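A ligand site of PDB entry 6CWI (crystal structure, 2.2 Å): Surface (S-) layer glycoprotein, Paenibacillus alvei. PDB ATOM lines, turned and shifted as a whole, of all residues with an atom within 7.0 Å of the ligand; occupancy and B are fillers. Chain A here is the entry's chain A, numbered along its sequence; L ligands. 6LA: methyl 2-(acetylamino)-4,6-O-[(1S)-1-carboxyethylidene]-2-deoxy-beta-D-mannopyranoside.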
ATOM      1  N   ARG A  41       8.488   5.748   2.271  1.00  0.00           N
ATOM      2  CA  ARG A  41       8.289   5.241   0.896  1.00  0.00           C
ATOM      3  C   ARG A  41       8.945   3.856   0.716  1.00  0.00           C
ATOM      4  O   ARG A  41       8.446   3.005  -0.061  1.00  0.00           O
ATOM      5  CB  ARG A  41       8.813   6.253  -0.151  1.00  0.00           C
ATOM      6  CG  ARG A  41       7.959   7.483  -0.207  1.00  0.00           C
ATOM      7  CD  ARG A  41       8.514   8.680  -0.967  1.00  0.00           C
ATOM      8  NE  ARG A  41       9.021   8.348  -2.292  1.00  0.00           N
ATOM      9  CZ  ARG A  41       8.307   8.077  -3.380  1.00  0.00           C
ATOM     10  NH1 ARG A  41       6.968   8.085  -3.332  1.00  0.00           N
ATOM     11  NH2 ARG A  41       8.933   7.747  -4.508  1.00  0.00           N
ATOM     12  N   TYR A  63      18.751   3.644  -8.273  1.00  0.00           N
ATOM     13  CA  TYR A  63      18.580   5.004  -7.789  1.00  0.00           C
ATOM     14  C   TYR A  63      19.860   5.484  -7.108  1.00  0.00           C
ATOM     15  O   TYR A  63      20.605   4.671  -6.567  1.00  0.00           O
ATOM     16  CB  TYR A  63      17.408   5.089  -6.806  1.00  0.00           C
ATOM     17  CG  TYR A  63      16.021   4.804  -7.397  1.00  0.00           C
ATOM     18  CD1 TYR A  63      15.403   5.726  -8.242  1.00  0.00           C
ATOM     19  CD2 TYR A  63      15.345   3.619  -7.095  1.00  0.00           C
ATOM     20  CE1 TYR A  63      14.136   5.480  -8.766  1.00  0.00           C
ATOM     21  CE2 TYR A  63      14.091   3.352  -7.616  1.00  0.00           C
ATOM     22  CZ  TYR A  63      13.466   4.294  -8.456  1.00  0.00           C
ATOM     23  OH  TYR A  63      12.229   4.074  -9.033  1.00  0.00           O
ATOM     24  N   GLY A  85       6.512  -0.954 -12.670  1.00  0.00           N
ATOM     25  CA  GLY A  85       5.823   0.267 -13.133  1.00  0.00           C
ATOM     26  C   GLY A  85       4.949   0.995 -12.076  1.00  0.00           C
ATOM     27  O   GLY A  85       4.321   1.972 -12.398  1.00  0.00           O
ATOM     28  N   LEU A  86       4.914   0.508 -10.845  1.00  0.00           N
ATOM     29  CA  LEU A  86       4.104   1.078  -9.790  1.00  0.00           C
ATOM     30  C   LEU A  86       4.735   2.321  -9.236  1.00  0.00           C
ATOM     31  O   LEU A  86       3.996   3.266  -8.914  1.00  0.00           O
ATOM     32  CB  LEU A  86       3.956   0.128  -8.639  1.00  0.00           C
ATOM     33  CG  LEU A  86       3.377  -1.187  -9.027  1.00  0.00           C
ATOM     34  CD1 LEU A  86       3.021  -1.950  -7.755  1.00  0.00           C
ATOM     35  CD2 LEU A  86       2.177  -0.998  -9.956  1.00  0.00           C
ATOM     36  N   MET A  87       6.069   2.338  -9.113  1.00  0.00           N
ATOM     37  CA  MET A  87       6.813   3.555  -8.658  1.00  0.00           C
ATOM     38  C   MET A  87       7.995   3.894  -9.580  1.00  0.00           C
ATOM     39  O   MET A  87       8.550   3.051 -10.219  1.00  0.00           O
ATOM     40  CB  MET A  87       7.287   3.430  -7.217  1.00  0.00           C
ATOM     41  CG  MET A  87       6.168   3.066  -6.230  1.00  0.00           C
ATOM     42  SD  MET A  87       6.614   3.053  -4.467  1.00  0.00           S
ATOM     43  CE  MET A  87       6.764   4.816  -4.125  1.00  0.00           C
ATOM     44  N   GLN A  88       8.308   5.186  -9.629  1.00  0.00           N
ATOM     45  CA  GLN A  88       9.277   5.821 -10.530  1.00  0.00           C
ATOM     46  C   GLN A  88      10.271   6.697  -9.775  1.00  0.00           C
ATOM     47  O   GLN A  88      11.258   7.147 -10.338  1.00  0.00           O
ATOM     48  CB  GLN A  88       8.440   6.859 -11.310  1.00  0.00           C
ATOM     49  CG  GLN A  88       8.559   6.938 -12.793  1.00  0.00           C
ATOM     50  CD  GLN A  88       7.737   8.092 -13.315  1.00  0.00           C
ATOM     51  OE1 GLN A  88       7.021   8.755 -12.556  1.00  0.00           O
ATOM     52  NE2 GLN A  88       7.788   8.314 -14.616  1.00  0.00           N
ATOM     53  N   GLY A  89       9.940   7.077  -8.539  1.00  0.00           N
ATOM     54  CA  GLY A  89      10.726   8.096  -7.834  1.00  0.00           C
ATOM     55  C   GLY A  89      10.276   9.496  -8.168  1.00  0.00           C
ATOM     56  O   GLY A  89       9.307   9.704  -8.913  1.00  0.00           O
ATOM     57  N   LYS A  90      10.995  10.476  -7.649  1.00  0.00           N
ATOM     58  CA  LYS A  90      10.562  11.882  -7.684  1.00  0.00           C
ATOM     59  C   LYS A  90      11.296  12.700  -8.722  1.00  0.00           C
ATOM     60  O   LYS A  90      10.792  13.731  -9.122  1.00  0.00           O
ATOM     61  CB  LYS A  90      10.682  12.539  -6.311  1.00  0.00           C
ATOM     62  CG  LYS A  90      10.466  11.597  -5.138  1.00  0.00           C
ATOM     63  CD  LYS A  90       9.212  11.867  -4.333  1.00  0.00           C
ATOM     64  CE  LYS A  90       9.470  12.863  -3.237  1.00  0.00           C
ATOM     65  NZ  LYS A  90       8.750  12.573  -1.969  1.00  0.00           N
ATOM     66  N   ASP A  91      12.513  12.313  -9.138  1.00  0.00           N
ATOM     67  CA  ASP A  91      12.984  12.739 -10.464  1.00  0.00           C
ATOM     68  C   ASP A  91      13.945  11.849 -11.191  1.00  0.00           C
ATOM     69  O   ASP A  91      14.849  11.190 -10.640  1.00  0.00           O
ATOM     70  CB  ASP A  91      13.487  14.181 -10.547  1.00  0.00           C
ATOM     71  CG  ASP A  91      14.796  14.365  -9.910  1.00  0.00           C
ATOM     72  OD1 ASP A  91      15.026  13.610  -8.936  1.00  0.00           O
ATOM     73  OD2 ASP A  91      15.554  15.256 -10.339  1.00  0.00           O
ATOM     74  N   LEU A  92      13.655  11.838 -12.472  1.00  0.00           N
ATOM     75  CA  LEU A  92      14.177  10.891 -13.380  1.00  0.00           C
ATOM     76  C   LEU A  92      15.549  11.335 -13.704  1.00  0.00           C
ATOM     77  O   LEU A  92      16.424  10.499 -13.859  1.00  0.00           O
ATOM     78  CB  LEU A  92      13.296  10.815 -14.614  1.00  0.00           C
ATOM     79  CG  LEU A  92      11.863  10.399 -14.261  1.00  0.00           C
ATOM     80  CD1 LEU A  92      11.015  10.189 -15.509  1.00  0.00           C
ATOM     81  CD2 LEU A  92      11.855   9.145 -13.370  1.00  0.00           C
ATOM     82  N   ILE A  96      16.260  10.023  -8.101  1.00  0.00           N
ATOM     83  CA  ILE A  96      15.985  10.111  -6.688  1.00  0.00           C
ATOM     84  C   ILE A  96      14.594   9.536  -6.441  1.00  0.00           C
ATOM     85  O   ILE A  96      13.621  10.001  -7.040  1.00  0.00           O
ATOM     86  CB  ILE A  96      16.027  11.578  -6.194  1.00  0.00           C
ATOM     87  CG1 ILE A  96      17.438  12.152  -6.394  1.00  0.00           C
ATOM     88  CG2 ILE A  96      15.576  11.666  -4.737  1.00  0.00           C
ATOM     89  CD1 ILE A  96      18.496  11.421  -5.612  1.00  0.00           C
ATOM     90  N   PHE A  97      14.559   8.516  -5.581  1.00  0.00           N
ATOM     91  CA  PHE A  97      13.360   7.855  -5.117  1.00  0.00           C
ATOM     92  C   PHE A  97      12.852   8.478  -3.850  1.00  0.00           C
ATOM     93  O   PHE A  97      11.668   8.464  -3.617  1.00  0.00           O
ATOM     94  CB  PHE A  97      13.684   6.400  -4.762  1.00  0.00           C
ATOM     95  CG  PHE A  97      12.480   5.553  -4.507  1.00  0.00           C
ATOM     96  CD1 PHE A  97      11.671   5.152  -5.550  1.00  0.00           C
ATOM     97  CD2 PHE A  97      12.161   5.179  -3.217  1.00  0.00           C
ATOM     98  CE1 PHE A  97      10.545   4.377  -5.318  1.00  0.00           C
ATOM     99  CE2 PHE A  97      11.064   4.371  -2.970  1.00  0.00           C
ATOM    100  CZ  PHE A  97      10.242   3.982  -4.017  1.00  0.00           C
ATOM    101  N   ILE A 103       5.271   8.304   2.502  1.00  0.00           N
ATOM    102  CA  ILE A 103       4.374   8.092   1.380  1.00  0.00           C
ATOM    103  C   ILE A 103       3.170   9.005   1.550  1.00  0.00           C
ATOM    104  O   ILE A 103       2.692   9.147   2.644  1.00  0.00           O
ATOM    105  CB  ILE A 103       4.024   6.578   1.252  1.00  0.00           C
ATOM    106  CG1 ILE A 103       3.295   6.272  -0.055  1.00  0.00           C
ATOM    107  CG2 ILE A 103       3.255   6.070   2.470  1.00  0.00           C
ATOM    108  CD1 ILE A 103       4.176   6.283  -1.297  1.00  0.00           C
ATOM    109  N   THR A 104       2.677   9.625   0.478  1.00  0.00           N
ATOM    110  CA  THR A 104       1.512  10.481   0.571  1.00  0.00           C
ATOM    111  C   THR A 104       0.292   9.816  -0.002  1.00  0.00           C
ATOM    112  O   THR A 104       0.404   8.887  -0.787  1.00  0.00           O
ATOM    113  CB  THR A 104       1.702  11.809  -0.184  1.00  0.00           C
ATOM    114  OG1 THR A 104       1.810  11.570  -1.567  1.00  0.00           O
ATOM    115  CG2 THR A 104       2.961  12.538   0.307  1.00  0.00           C
ATOM    116  N   GLU A 106      -1.785  10.691  -2.288  1.00  0.00           N
ATOM    117  CA  GLU A 106      -1.846  10.729  -3.763  1.00  0.00           C
ATOM    118  C   GLU A 106      -0.805   9.792  -4.413  1.00  0.00           C
ATOM    119  O   GLU A 106      -1.085   9.182  -5.452  1.00  0.00           O
ATOM    120  CB  GLU A 106      -1.732  12.172  -4.308  1.00  0.00           C
ATOM    121  CG  GLU A 106      -0.363  12.861  -4.117  1.00  0.00           C
ATOM    122  CD  GLU A 106      -0.349  14.338  -4.548  1.00  0.00           C
ATOM    123  OE1 GLU A 106      -1.395  14.916  -4.951  1.00  0.00           O
ATOM    124  OE2 GLU A 106       0.704  14.970  -4.405  1.00  0.00           O
ATOM    125  N   GLU A 107       0.382   9.677  -3.793  1.00  0.00           N
ATOM    126  CA  GLU A 107       1.390   8.689  -4.209  1.00  0.00           C
ATOM    127  C   GLU A 107       0.886   7.270  -4.041  1.00  0.00           C
ATOM    128  O   GLU A 107       0.917   6.477  -4.994  1.00  0.00           O
ATOM    129  CB  GLU A 107       2.682   8.809  -3.385  1.00  0.00           C
ATOM    130  CG  GLU A 107       3.494  10.082  -3.641  1.00  0.00           C
ATOM    131  CD  GLU A 107       4.614  10.337  -2.591  1.00  0.00           C
ATOM    132  OE1 GLU A 107       4.812   9.536  -1.622  1.00  0.00           O
ATOM    133  OE2 GLU A 107       5.336  11.349  -2.787  1.00  0.00           O
ATOM    134  N   ALA A 108       0.415   6.930  -2.843  1.00  0.00           N
ATOM    135  CA  ALA A 108      -0.147   5.619  -2.656  1.00  0.00           C
ATOM    136  C   ALA A 108      -1.234   5.379  -3.714  1.00  0.00           C
ATOM    137  O   ALA A 108      -1.375   4.264  -4.224  1.00  0.00           O
ATOM    138  CB  ALA A 108      -0.703   5.465  -1.238  1.00  0.00           C
ATOM    139  N   SER A 109      -2.046   6.419  -3.962  1.00  0.00           N
ATOM    140  CA  SER A 109      -3.160   6.326  -4.924  1.00  0.00           C
ATOM    141  C   SER A 109      -2.644   5.921  -6.294  1.00  0.00           C
ATOM    142  O   SER A 109      -3.167   4.996  -6.928  1.00  0.00           O
ATOM    143  CB  SER A 109      -3.963   7.669  -5.033  1.00  0.00           C
ATOM    144  OG  SER A 109      -4.701   7.943  -3.847  1.00  0.00           O
ATOM    145  N   LYS A 110      -1.617   6.620  -6.753  1.00  0.00           N
ATOM    146  CA  LYS A 110      -0.955   6.253  -8.000  1.00  0.00           C
ATOM    147  C   LYS A 110      -0.656   4.741  -8.002  1.00  0.00           C
ATOM    148  O   LYS A 110      -1.037   4.033  -8.957  1.00  0.00           O
ATOM    149  CB  LYS A 110       0.352   7.030  -8.195  1.00  0.00           C
ATOM    150  CG  LYS A 110       1.038   6.658  -9.495  1.00  0.00           C
ATOM    151  CD  LYS A 110       2.376   7.310  -9.692  1.00  0.00           C
ATOM    152  CE  LYS A 110       3.280   6.423 -10.561  1.00  0.00           C
ATOM    153  NZ  LYS A 110       4.532   7.078 -10.999  1.00  0.00           N
ATOM    154  N   THR A 111       0.034   4.258  -6.969  1.00  0.00           N
ATOM    155  CA  THR A 111       0.554   2.902  -6.976  1.00  0.00           C
ATOM    156  C   THR A 111      -0.550   1.864  -7.081  1.00  0.00           C
ATOM    157  O   THR A 111      -0.460   0.919  -7.840  1.00  0.00           O
ATOM    158  CB  THR A 111       1.471   2.621  -5.783  1.00  0.00           C
ATOM    159  OG1 THR A 111       0.718   2.534  -4.568  1.00  0.00           O
ATOM    160  CG2 THR A 111       2.535   3.704  -5.674  1.00  0.00           C
ATOM    161  N   TRP A 131       0.131  16.150 -11.346  1.00  0.00           N
ATOM    162  CA  TRP A 131       0.485  14.830 -11.852  1.00  0.00           C
ATOM    163  C   TRP A 131      -0.436  13.719 -11.280  1.00  0.00           C
ATOM    164  O   TRP A 131      -0.622  12.686 -11.911  1.00  0.00           O
ATOM    165  CB  TRP A 131       1.950  14.505 -11.556  1.00  0.00           C
ATOM    166  CG  TRP A 131       2.253  14.328 -10.089  1.00  0.00           C
ATOM    167  CD1 TRP A 131       2.798  15.246  -9.256  1.00  0.00           C
ATOM    168  CD2 TRP A 131       2.049  13.133  -9.307  1.00  0.00           C
ATOM    169  NE1 TRP A 131       2.917  14.722  -7.984  1.00  0.00           N
ATOM    170  CE2 TRP A 131       2.489  13.421  -7.980  1.00  0.00           C
ATOM    171  CE3 TRP A 131       1.556  11.851  -9.606  1.00  0.00           C
ATOM    172  CZ2 TRP A 131       2.434  12.488  -6.948  1.00  0.00           C
ATOM    173  CZ3 TRP A 131       1.494  10.929  -8.569  1.00  0.00           C
ATOM    174  CH2 TRP A 131       1.933  11.257  -7.251  1.00  0.00           C
ATOM    175  N   TYR A 135      -5.122  10.044 -10.737  1.00  0.00           N
ATOM    176  CA  TYR A 135      -4.835   8.908  -9.878  1.00  0.00           C
ATOM    177  C   TYR A 135      -5.658   8.972  -8.598  1.00  0.00           C
ATOM    178  O   TYR A 135      -6.282   7.984  -8.201  1.00  0.00           O
ATOM    179  CB  TYR A 135      -3.351   8.885  -9.484  1.00  0.00           C
ATOM    180  CG  TYR A 135      -2.423   8.521 -10.619  1.00  0.00           C
ATOM    181  CD1 TYR A 135      -2.593   7.343 -11.363  1.00  0.00           C
ATOM    182  CD2 TYR A 135      -1.323   9.328 -10.916  1.00  0.00           C
ATOM    183  CE1 TYR A 135      -1.695   7.015 -12.404  1.00  0.00           C
ATOM    184  CE2 TYR A 135      -0.435   9.012 -11.939  1.00  0.00           C
ATOM    185  CZ  TYR A 135      -0.620   7.875 -12.695  1.00  0.00           C
ATOM    186  OH  TYR A 135       0.306   7.626 -13.691  1.00  0.00           O
HETATM  187  C8  6LA L   1       9.166  11.327 -11.733  1.00  0.00           C
HETATM  188  C7  6LA L   1       7.810  11.871 -11.302  1.00  0.00           C
HETATM  189  O7  6LA L   1       7.127  12.572 -12.019  1.00  0.00           O
HETATM  190  N2  6LA L   1       7.406  11.484 -10.101  1.00  0.00           N
HETATM  191  C2  6LA L   1       6.128  11.961  -9.557  1.00  0.00           C
HETATM  192  C3  6LA L   1       5.175  10.784  -9.349  1.00  0.00           C
HETATM  193  O3  6LA L   1       5.005  10.104 -10.667  1.00  0.00           O
HETATM  194  C4  6LA L   1       5.790   9.898  -8.297  1.00  0.00           C
HETATM  195  O4  6LA L   1       4.860   8.962  -7.974  1.00  0.00           O
HETATM  196  CAB 6LA L   1       5.403   8.134  -6.932  1.00  0.00           C
HETATM  197  CAK 6LA L   1       4.328   7.106  -6.554  1.00  0.00           C
HETATM  198  CAL 6LA L   1       6.564   7.376  -7.544  1.00  0.00           C
HETATM  199  OAN 6LA L   1       7.530   6.966  -6.819  1.00  0.00           O
HETATM  200  OAM 6LA L   1       6.363   7.085  -8.764  1.00  0.00           O
HETATM  201  O6  6LA L   1       5.770   8.839  -5.741  1.00  0.00           O
HETATM  202  C6  6LA L   1       6.736   9.863  -5.989  1.00  0.00           C
HETATM  203  C5  6LA L   1       6.110  10.720  -7.035  1.00  0.00           C
HETATM  204  O5  6LA L   1       7.083  11.762  -7.370  1.00  0.00           O
HETATM  205  C1  6LA L   1       6.456  12.673  -8.281  1.00  0.00           C
HETATM  206  O1  6LA L   1       7.352  13.732  -8.625  1.00  0.00           O
HETATM  207  CAU 6LA L   1       7.765  14.501  -7.486  1.00  0.00           C
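N of Gln 88 is in hydrogen-bond range of OAM of the ligand, at 2.9 Å. OAM of the ligand lies within salt-bridge range of NZ of Lys 110 (2.9 Å). N2 of the ligand is in hydrogen-bond range of O of Gly 89 (2.9 Å). An oxygen (OAN) of the ligand sits at hydrogen-bond distance from the backbone NH of Gly 89, 3.0 Å away. The guanidinium group (NH2) of Arg 41 is in salt-bridge range of an oxygen (OAN) of the ligand, at 2.8 Å. O3 of the ligand lies within hydrogen-bond range of OE1 of Gln 88, 3.1 Å away.
NH1 of Arg 41 is in salt-bridge range of OE1 of Glu 107 (3.1 Å). O of Phe 97 sits at hydrogen-bond distance from NE of Arg 41. OG1 of Thr 111 sits at hydrogen-bond distance from O of Ala 108, 2.7 Å away. The side-chain amino group (NZ) of Lys 90 lies within salt-bridge range of the side-chain carboxylate (OE2) of Glu 107, 3.7 Å away. The backbone NH (N) of Thr 104 sits at hydrogen-bond distance from the side-chain carboxylate (OE1) of Glu 107 (3.0 Å). The side-chain amino group of Lys 110 sits at hydrogen-bond distance from the side-chain amide oxygen of Gln 88 (3.4 Å). OH of Tyr 63 sits close to O of Gln 88 (3.5 Å). N of Lys 90 lies within hydrogen-bond range of O of Ile 96 (2.7 Å).
The backbone carbonyl oxygen (O) of Lys 90 lies close to an oxygen (O1) of the ligand, at 3.5 Å. Met 87 touches the ligand. Leu 92 touches the ligand. Glu 107 touches the ligand. Thr 111 touches the ligand (CG2 to CAK, 3.9 Å). Trp 131 touches the ligand. Hydrophobic or aromatic side chains within 4 Å of the ligand: Met 87, Leu 92 and Trp 131. Of the 22 residues printed, 10 come within 4 Å of the ligand. The nearest printed residue that does not touch the ligand is Phe 97 (4.2 Å).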
